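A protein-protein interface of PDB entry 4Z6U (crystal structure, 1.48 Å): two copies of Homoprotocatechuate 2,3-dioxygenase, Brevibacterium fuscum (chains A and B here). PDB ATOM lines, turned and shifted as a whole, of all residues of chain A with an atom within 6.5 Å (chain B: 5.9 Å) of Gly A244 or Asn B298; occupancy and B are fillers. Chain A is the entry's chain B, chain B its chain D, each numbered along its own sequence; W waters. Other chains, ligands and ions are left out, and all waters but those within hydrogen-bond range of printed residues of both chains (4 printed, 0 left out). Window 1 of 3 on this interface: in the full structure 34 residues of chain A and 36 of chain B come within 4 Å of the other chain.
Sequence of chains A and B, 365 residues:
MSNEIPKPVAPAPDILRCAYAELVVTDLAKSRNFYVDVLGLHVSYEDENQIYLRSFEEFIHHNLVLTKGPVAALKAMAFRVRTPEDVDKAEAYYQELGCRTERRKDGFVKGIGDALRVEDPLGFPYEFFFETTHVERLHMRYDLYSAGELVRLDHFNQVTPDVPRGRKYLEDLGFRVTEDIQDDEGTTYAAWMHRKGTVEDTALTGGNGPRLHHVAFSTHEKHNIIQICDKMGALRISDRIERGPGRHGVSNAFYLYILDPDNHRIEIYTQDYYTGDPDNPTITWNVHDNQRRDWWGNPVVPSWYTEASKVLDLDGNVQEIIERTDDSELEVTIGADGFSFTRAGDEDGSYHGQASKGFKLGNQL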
ATOM      1  N   CYS A 229      -9.641  27.466   3.607  1.00  0.00           N
ATOM      2  CA  CYS A 229     -10.267  26.270   4.178  1.00  0.00           C
ATOM      3  C   CYS A 229     -11.146  26.626   5.382  1.00  0.00           C
ATOM      4  O   CYS A 229     -12.280  26.166   5.514  1.00  0.00           O
ATOM      5  CB  CYS A 229      -9.189  25.258   4.646  1.00  0.00           C
ATOM      6  SG  CYS A 229      -8.135  24.599   3.347  1.00  0.00           S
ATOM      7  N   SER A 238     -17.627  23.067   3.325  1.00  0.00           N
ATOM      8  CA  SER A 238     -16.445  22.199   3.352  1.00  0.00           C
ATOM      9  C   SER A 238     -16.536  21.016   2.382  1.00  0.00           C
ATOM     10  O   SER A 238     -15.507  20.486   1.969  1.00  0.00           O
ATOM     11  CB  SER A 238     -16.155  21.677   4.745  1.00  0.00           C
ATOM     12  OG  SER A 238     -17.184  20.912   5.258  1.00  0.00           O
ATOM     13  N   ILE A 241     -14.418  21.570  -0.625  1.00  0.00           N
ATOM     14  CA  ILE A 241     -12.975  21.295  -0.536  1.00  0.00           C
ATOM     15  C   ILE A 241     -12.762  19.865  -1.008  1.00  0.00           C
ATOM     16  O   ILE A 241     -13.263  18.914  -0.397  1.00  0.00           O
ATOM     17  CB  ILE A 241     -12.414  21.449   0.895  1.00  0.00           C
ATOM     18  CG1 ILE A 241     -12.656  22.880   1.425  1.00  0.00           C
ATOM     19  CG2 ILE A 241     -10.936  21.027   0.921  1.00  0.00           C
ATOM     20  CD1 ILE A 241     -12.296  23.067   2.861  1.00  0.00           C
ATOM     21  N   GLU A 242     -12.095  19.725  -2.159  1.00  0.00           N
ATOM     22  CA  GLU A 242     -11.909  18.406  -2.734  1.00  0.00           C
ATOM     23  C   GLU A 242     -10.724  17.661  -2.149  1.00  0.00           C
ATOM     24  O   GLU A 242     -10.800  16.456  -1.885  1.00  0.00           O
ATOM     25  CB  GLU A 242     -11.724  18.499  -4.257  1.00  0.00           C
ATOM     26  CG  GLU A 242     -11.683  17.122  -4.941  1.00  0.00           C
ATOM     27  CD  GLU A 242     -11.181  17.202  -6.369  1.00  0.00           C
ATOM     28  OE1 GLU A 242     -10.341  18.101  -6.672  1.00  0.00           O
ATOM     29  OE2 GLU A 242     -11.666  16.363  -7.176  1.00  0.00           O
ATOM     30  N   ARG A 243      -9.603  18.367  -2.041  1.00  0.00           N
ATOM     31  CA  ARG A 243      -8.323  17.713  -1.734  1.00  0.00           C
ATOM     32  C   ARG A 243      -7.401  18.737  -1.115  1.00  0.00           C
ATOM     33  O   ARG A 243      -7.272  19.839  -1.629  1.00  0.00           O
ATOM     34  CB  ARG A 243      -7.707  17.108  -3.010  1.00  0.00           C
ATOM     35  CG  ARG A 243      -6.333  16.501  -2.762  1.00  0.00           C
ATOM     36  CD  ARG A 243      -5.723  15.880  -3.999  1.00  0.00           C
ATOM     37  NE  ARG A 243      -4.293  15.714  -3.752  1.00  0.00           N
ATOM     38  CZ  ARG A 243      -3.344  15.893  -4.630  1.00  0.00           C
ATOM     39  NH1 ARG A 243      -3.609  16.056  -5.931  1.00  0.00           N
ATOM     40  NH2 ARG A 243      -2.113  15.877  -4.211  1.00  0.00           N
ATOM     41  N   GLY A 244      -6.755  18.376   0.007  1.00  0.00           N
ATOM     42  CA  GLY A 244      -5.806  19.236   0.643  1.00  0.00           C
ATOM     43  C   GLY A 244      -6.355  19.777   1.947  1.00  0.00           C
ATOM     44  O   GLY A 244      -7.375  19.313   2.447  1.00  0.00           O
ATOM     45  N   PRO A 245      -5.672  20.776   2.504  1.00  0.00           N
ATOM     46  CA  PRO A 245      -4.445  21.338   1.994  1.00  0.00           C
ATOM     47  C   PRO A 245      -3.260  20.369   2.171  1.00  0.00           C
ATOM     48  O   PRO A 245      -3.285  19.445   3.031  1.00  0.00           O
ATOM     49  CB  PRO A 245      -4.270  22.597   2.835  1.00  0.00           C
ATOM     50  CG  PRO A 245      -4.871  22.242   4.151  1.00  0.00           C
ATOM     51  CD  PRO A 245      -6.036  21.361   3.792  1.00  0.00           C
ATOM     52  N   GLY A 246      -2.232  20.601   1.371  1.00  0.00           N
ATOM     53  CA  GLY A 246      -1.052  19.753   1.444  1.00  0.00           C
ATOM     54  C   GLY A 246       0.199  20.434   0.952  1.00  0.00           C
ATOM     55  O   GLY A 246       0.188  21.611   0.602  1.00  0.00           O
ATOM     56  N   TYR A 255      -0.648  23.680  -1.266  1.00  0.00           N
ATOM     57  CA  TYR A 255      -1.761  23.596  -2.219  1.00  0.00           C
ATOM     58  C   TYR A 255      -3.096  23.260  -1.579  1.00  0.00           C
ATOM     59  O   TYR A 255      -3.158  22.737  -0.452  1.00  0.00           O
ATOM     60  CB  TYR A 255      -1.469  22.568  -3.301  1.00  0.00           C
ATOM     61  CG  TYR A 255      -1.609  21.132  -2.820  1.00  0.00           C
ATOM     62  CD1 TYR A 255      -0.509  20.432  -2.351  1.00  0.00           C
ATOM     63  CD2 TYR A 255      -2.834  20.466  -2.838  1.00  0.00           C
ATOM     64  CE1 TYR A 255      -0.626  19.118  -1.901  1.00  0.00           C
ATOM     65  CE2 TYR A 255      -2.970  19.153  -2.389  1.00  0.00           C
ATOM     66  CZ  TYR A 255      -1.844  18.469  -1.931  1.00  0.00           C
ATOM     67  OH  TYR A 255      -2.020  17.150  -1.478  1.00  0.00           O
ATOM     68  N   LEU A 256      -4.153  23.556  -2.328  1.00  0.00           N
ATOM     69  CA  LEU A 256      -5.523  23.232  -1.965  1.00  0.00           C
ATOM     70  C   LEU A 256      -6.322  23.124  -3.274  1.00  0.00           C
ATOM     71  O   LEU A 256      -6.130  23.937  -4.173  1.00  0.00           O
ATOM     72  CB  LEU A 256      -6.127  24.356  -1.118  1.00  0.00           C
ATOM     73  CG  LEU A 256      -7.600  24.185  -0.742  1.00  0.00           C
ATOM     74  CD1 LEU A 256      -7.806  23.019   0.197  1.00  0.00           C
ATOM     75  CD2 LEU A 256      -8.102  25.495  -0.161  1.00  0.00           C
ATOM     76  N   TYR A 257      -7.199  22.153  -3.352  1.00  0.00           N
ATOM     77  CA  TYR A 257      -8.158  22.064  -4.448  1.00  0.00           C
ATOM     78  C   TYR A 257      -9.584  22.186  -3.967  1.00  0.00           C
ATOM     79  O   TYR A 257     -10.026  21.445  -3.091  1.00  0.00           O
ATOM     80  CB  TYR A 257      -8.018  20.757  -5.199  1.00  0.00           C
ATOM     81  CG  TYR A 257      -6.657  20.545  -5.821  1.00  0.00           C
ATOM     82  CD1 TYR A 257      -6.325  21.088  -7.063  1.00  0.00           C
ATOM     83  CD2 TYR A 257      -5.678  19.787  -5.155  1.00  0.00           C
ATOM     84  CE1 TYR A 257      -5.055  20.893  -7.595  1.00  0.00           C
ATOM     85  CE2 TYR A 257      -4.422  19.603  -5.684  1.00  0.00           C
ATOM     86  CZ  TYR A 257      -4.114  20.127  -6.925  1.00  0.00           C
ATOM     87  OH  TYR A 257      -2.828  19.895  -7.450  1.00  0.00           O
ATOM     88  N   ASP A 294       1.242  14.336  -2.849  1.00  0.00           N
ATOM     89  CA  ASP A 294       1.241  14.883  -1.491  1.00  0.00           C
ATOM     90  C   ASP A 294       2.476  14.360  -0.746  1.00  0.00           C
ATOM     91  O   ASP A 294       2.646  13.150  -0.514  1.00  0.00           O
ATOM     92  CB  ASP A 294      -0.027  14.508  -0.741  1.00  0.00           C
ATOM     93  CG  ASP A 294      -0.116  15.274   0.580  1.00  0.00           C
ATOM     94  OD1 ASP A 294      -0.537  16.457   0.534  1.00  0.00           O
ATOM     95  OD2 ASP A 294       0.279  14.731   1.646  1.00  0.00           O
ATOM     96  N   VAL A 301      -7.597  11.803  -3.499  1.00  0.00           N
ATOM     97  CA  VAL A 301      -8.991  11.460  -3.656  1.00  0.00           C
ATOM     98  C   VAL A 301      -9.275  11.022  -5.119  1.00  0.00           C
ATOM     99  O   VAL A 301      -8.777  11.639  -6.068  1.00  0.00           O
ATOM    100  CB  VAL A 301      -9.896  12.637  -3.189  1.00  0.00           C
ATOM    101  CG1 VAL A 301      -9.563  13.010  -1.736  1.00  0.00           C
ATOM    102  CG2 VAL A 301      -9.719  13.859  -4.062  1.00  0.00           C
ATOM    103  N   PRO B 245      -2.238  17.563   8.386  1.00  0.00           N
ATOM    104  CA  PRO B 245      -2.641  18.604   9.315  1.00  0.00           C
ATOM    105  C   PRO B 245      -4.061  19.073   9.021  1.00  0.00           C
ATOM    106  O   PRO B 245      -4.590  18.897   7.912  1.00  0.00           O
ATOM    107  CB  PRO B 245      -1.616  19.716   9.058  1.00  0.00           C
ATOM    108  CG  PRO B 245      -1.303  19.553   7.611  1.00  0.00           C
ATOM    109  CD  PRO B 245      -1.302  18.080   7.374  1.00  0.00           C
ATOM    110  N   TYR B 255      -3.878  21.451  13.916  1.00  0.00           N
ATOM    111  CA  TYR B 255      -3.421  20.191  14.498  1.00  0.00           C
ATOM    112  C   TYR B 255      -2.709  19.268  13.524  1.00  0.00           C
ATOM    113  O   TYR B 255      -2.849  19.354  12.288  1.00  0.00           O
ATOM    114  CB  TYR B 255      -4.587  19.445  15.157  1.00  0.00           C
ATOM    115  CG  TYR B 255      -5.502  18.760  14.140  1.00  0.00           C
ATOM    116  CD1 TYR B 255      -5.231  17.497  13.668  1.00  0.00           C
ATOM    117  CD2 TYR B 255      -6.619  19.405  13.657  1.00  0.00           C
ATOM    118  CE1 TYR B 255      -6.057  16.907  12.737  1.00  0.00           C
ATOM    119  CE2 TYR B 255      -7.460  18.819  12.714  1.00  0.00           C
ATOM    120  CZ  TYR B 255      -7.163  17.568  12.263  1.00  0.00           C
ATOM    121  OH  TYR B 255      -7.950  16.935  11.337  1.00  0.00           O
ATOM    122  N   ASN B 290     -19.768  16.458  10.118  1.00  0.00           N
ATOM    123  CA  ASN B 290     -18.475  16.166   9.503  1.00  0.00           C
ATOM    124  C   ASN B 290     -17.459  17.295   9.637  1.00  0.00           C
ATOM    125  O   ASN B 290     -16.341  17.133   9.168  1.00  0.00           O
ATOM    126  CB  ASN B 290     -18.626  15.813   8.012  1.00  0.00           C
ATOM    127  CG  ASN B 290     -17.365  15.223   7.425  1.00  0.00           C
ATOM    128  OD1 ASN B 290     -16.799  14.240   7.954  1.00  0.00           O
ATOM    129  ND2 ASN B 290     -16.906  15.810   6.319  1.00  0.00           N
ATOM    130  N   ASP B 294     -12.431  17.497  12.007  1.00  0.00           N
ATOM    131  CA  ASP B 294     -11.720  18.290  11.048  1.00  0.00           C
ATOM    132  C   ASP B 294     -12.740  19.251  10.449  1.00  0.00           C
ATOM    133  O   ASP B 294     -13.684  18.834   9.770  1.00  0.00           O
ATOM    134  CB  ASP B 294     -11.107  17.437   9.945  1.00  0.00           C
ATOM    135  CG  ASP B 294     -10.198  18.260   9.066  1.00  0.00           C
ATOM    136  OD1 ASP B 294      -9.018  18.484   9.482  1.00  0.00           O
ATOM    137  OD2 ASP B 294     -10.662  18.711   7.997  1.00  0.00           O
ATOM    138  N   TRP B 295     -12.530  20.529  10.716  1.00  0.00           N
ATOM    139  CA  TRP B 295     -13.430  21.609  10.304  1.00  0.00           C
ATOM    140  C   TRP B 295     -13.564  21.697   8.797  1.00  0.00           C
ATOM    141  O   TRP B 295     -14.570  22.207   8.306  1.00  0.00           O
ATOM    142  CB  TRP B 295     -12.850  22.902  10.866  1.00  0.00           C
ATOM    143  CG  TRP B 295     -13.562  24.164  10.600  1.00  0.00           C
ATOM    144  CD1 TRP B 295     -13.049  25.245   9.957  1.00  0.00           C
ATOM    145  CD2 TRP B 295     -14.848  24.568  11.090  1.00  0.00           C
ATOM    146  NE1 TRP B 295     -13.950  26.312   9.993  1.00  0.00           N
ATOM    147  CE2 TRP B 295     -15.061  25.907  10.679  1.00  0.00           C
ATOM    148  CE3 TRP B 295     -15.845  23.931  11.843  1.00  0.00           C
ATOM    149  CZ2 TRP B 295     -16.195  26.626  11.016  1.00  0.00           C
ATOM    150  CZ3 TRP B 295     -16.980  24.655  12.154  1.00  0.00           C
ATOM    151  CH2 TRP B 295     -17.143  25.978  11.746  1.00  0.00           C
ATOM    152  N   TRP B 296     -12.549  21.201   8.090  1.00  0.00           N
ATOM    153  CA  TRP B 296     -12.543  21.226   6.610  1.00  0.00           C
ATOM    154  C   TRP B 296     -13.213  20.005   6.024  1.00  0.00           C
ATOM    155  O   TRP B 296     -13.260  19.823   4.782  1.00  0.00           O
ATOM    156  CB  TRP B 296     -11.103  21.340   6.127  1.00  0.00           C
ATOM    157  CG  TRP B 296     -10.341  22.476   6.750  1.00  0.00           C
ATOM    158  CD1 TRP B 296     -10.825  23.678   7.245  1.00  0.00           C
ATOM    159  CD2 TRP B 296      -8.907  22.521   6.941  1.00  0.00           C
ATOM    160  NE1 TRP B 296      -9.783  24.416   7.725  1.00  0.00           N
ATOM    161  CE2 TRP B 296      -8.605  23.741   7.554  1.00  0.00           C
ATOM    162  CE3 TRP B 296      -7.867  21.605   6.700  1.00  0.00           C
ATOM    163  CZ2 TRP B 296      -7.295  24.102   7.883  1.00  0.00           C
ATOM    164  CZ3 TRP B 296      -6.579  21.981   6.963  1.00  0.00           C
ATOM    165  CH2 TRP B 296      -6.301  23.212   7.571  1.00  0.00           C
ATOM    166  N   GLY B 297     -13.664  19.102   6.893  1.00  0.00           N
ATOM    167  CA  GLY B 297     -14.406  17.934   6.436  1.00  0.00           C
ATOM    168  C   GLY B 297     -13.524  16.780   6.044  1.00  0.00           C
ATOM    169  O   GLY B 297     -14.024  15.773   5.548  1.00  0.00           O
ATOM    170  N   ASN B 298     -12.202  16.888   6.231  1.00  0.00           N
ATOM    171  CA  ASN B 298     -11.342  15.748   5.859  1.00  0.00           C
ATOM    172  C   ASN B 298     -11.634  14.536   6.739  1.00  0.00           C
ATOM    173  O   ASN B 298     -11.999  14.664   7.919  1.00  0.00           O
ATOM    174  CB  ASN B 298      -9.888  16.152   5.941  1.00  0.00           C
ATOM    175  CG  ASN B 298      -9.429  16.912   4.708  1.00  0.00           C
ATOM    176  OD1 ASN B 298      -9.916  16.665   3.610  1.00  0.00           O
ATOM    177  ND2 ASN B 298      -8.494  17.828   4.881  1.00  0.00           N
ATOM    178  N   PRO B 299     -11.525  13.342   6.144  1.00  0.00           N
ATOM    179  CA  PRO B 299     -11.920  12.136   6.839  1.00  0.00           C
ATOM    180  C   PRO B 299     -10.976  11.813   7.981  1.00  0.00           C
ATOM    181  O   PRO B 299      -9.771  12.105   7.925  1.00  0.00           O
ATOM    182  CB  PRO B 299     -11.851  11.062   5.736  1.00  0.00           C
ATOM    183  CG  PRO B 299     -10.847  11.586   4.790  1.00  0.00           C
ATOM    184  CD  PRO B 299     -11.065  13.067   4.775  1.00  0.00           C
ATOM    185  N   VAL B 300     -11.549  11.234   9.031  1.00  0.00           N
ATOM    186  CA  VAL B 300     -10.761  10.788  10.190  1.00  0.00           C
ATOM    187  C   VAL B 300     -10.329   9.360   9.972  1.00  0.00           C
ATOM    188  O   VAL B 300     -11.169   8.466   9.830  1.00  0.00           O
ATOM    189  CB  VAL B 300     -11.546  10.887  11.511  1.00  0.00           C
ATOM    190  CG1 VAL B 300     -10.720  10.376  12.668  1.00  0.00           C
ATOM    191  CG2 VAL B 300     -12.018  12.316  11.750  1.00  0.00           C
ATOM    192  N   SER B 356     -15.840  10.982   4.242  1.00  0.00           N
ATOM    193  CA  SER B 356     -15.862  12.126   3.346  1.00  0.00           C
ATOM    194  C   SER B 356     -14.806  11.986   2.243  1.00  0.00           C
ATOM    195  O   SER B 356     -13.883  11.152   2.337  1.00  0.00           O
ATOM    196  CB  SER B 356     -15.657  13.413   4.159  1.00  0.00           C
ATOM    197  OG  SER B 356     -14.472  13.278   4.934  1.00  0.00           O
ATOM    198  N   LYS B 357     -14.944  12.836   1.216  1.00  0.00           N
ATOM    199  CA  LYS B 357     -13.922  13.084   0.197  1.00  0.00           C
ATOM    200  C   LYS B 357     -13.703  11.899  -0.746  1.00  0.00           C
ATOM    201  O   LYS B 357     -12.793  11.932  -1.569  1.00  0.00           O
ATOM    202  CB  LYS B 357     -12.553  13.576   0.780  1.00  0.00           C
ATOM    203  CG  LYS B 357     -12.573  14.653   1.878  1.00  0.00           C
ATOM    204  CD  LYS B 357     -13.032  16.021   1.453  1.00  0.00           C
ATOM    205  CE  LYS B 357     -12.821  17.101   2.517  1.00  0.00           C
ATOM    206  NZ  LYS B 357     -13.831  18.201   2.346  1.00  0.00           N
HETATM  207  O   HOH W   1      -4.520  18.191   5.183  1.00  0.00           O
HETATM  208  O   HOH W   2     -13.278  15.261  -2.218  1.00  0.00           O
HETATM  209  O   HOH W   3     -17.908  18.304   5.001  1.00  0.00           O
HETATM  210  O   HOH W   4      -8.144  16.276   1.518  1.00  0.00           O
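The side-chain amino group (NZ) of Lys B357 is in hydrogen-bond range of the backbone carbonyl oxygen (O) of Ser A238 (2.9 Å).
NZ of Lys B357 sits at hydrogen-bond distance from O of Ile A241, at 2.9 Å.
O of Gly A244 is in hydrogen-bond range of ND2 of Asn B298 (3.1 Å).
N of Trp B296 lies close to OD2 of Asp B294 (3.1 Å).
The side-chain carboxylate (OD2) of Asp B294 sits at hydrogen-bond distance from the backbone NH (N) of Asn B298, 3.0 Å away.
The side-chain amino group (NZ) of Lys B357 sits at hydrogen-bond distance from the backbone carbonyl oxygen (O) of Trp B296, 3.0 Å away.
Trp B296 touches Cys A229.
Ser A238 touches Trp B295.
Ser A238 touches Trp B296 (CB to O, 3.4 Å).
Ile A241 touches Trp B296.
CD of Pro A245 touches CZ3 of Trp B296, 3.3 Å away.
Lys B357 touches Val A301.
Of the printed residues of chain B, Cys A229 touches Trp B296 (3.2 Å).
Printed residues of chain B within 4 Å of Ser A238: Trp B295 (3.9 Å), Trp B296 (3.4 Å) and Lys B357 (2.9 Å).
Of the printed residues of chain B, Ile A241 touches Trp B296 (3.9 Å) and Lys B357 (2.9 Å).
Gly A244 touches just one residue of chain B: Asn B298.
Printed residues of chain B within 4 Å of Val A301: Lys B357.
Asp B294 touches none of the printed residues of chain A.
Asn B298 touches just one residue of chain A: Gly A244 (3.1 Å).
Val B300 touches none of the printed residues of chain A.
The nearest residue of chain A that does not touch Asn B298 is Pro A245 (4.4 Å).
The nearest printed residue of chain B that does not touch Ile A241 is Asn B298 (5.2 Å).
Of the 12 printed residues of chain B, 4 touch a printed residue of chain A.
Hydrophobic or aromatic side chains of chain A within 4 Å of the printed part of chain B: Ile A241, Pro A245 and Val A301.
Among the printed residues, 9 pairs touch across the chains.
Among the printed residues, no Asp or Glu carboxylate lies within 4 Å of a Lys or Arg side-chain nitrogen of the other chain.
Positions printed for both chains: 245, 255 and 294.
Of the 9 pairs that touch across the chains among the printed residues, none has its exchanged pair printed and touching as well.
Water W3 bridges OG of Ser A238 (2.7 Å) and ND2 of Asn B290 (3.0 Å).
Water W4 lies within hydrogen-bond range of OD1 of Asn B298 and N of Gly A244.
Water W2 lies within hydrogen-bond range of the backbone carbonyl oxygen of Glu A242 and the backbone carbonyl oxygen of Lys B357.
Water W1 bridges O of Pro A245 and O of Pro B245.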
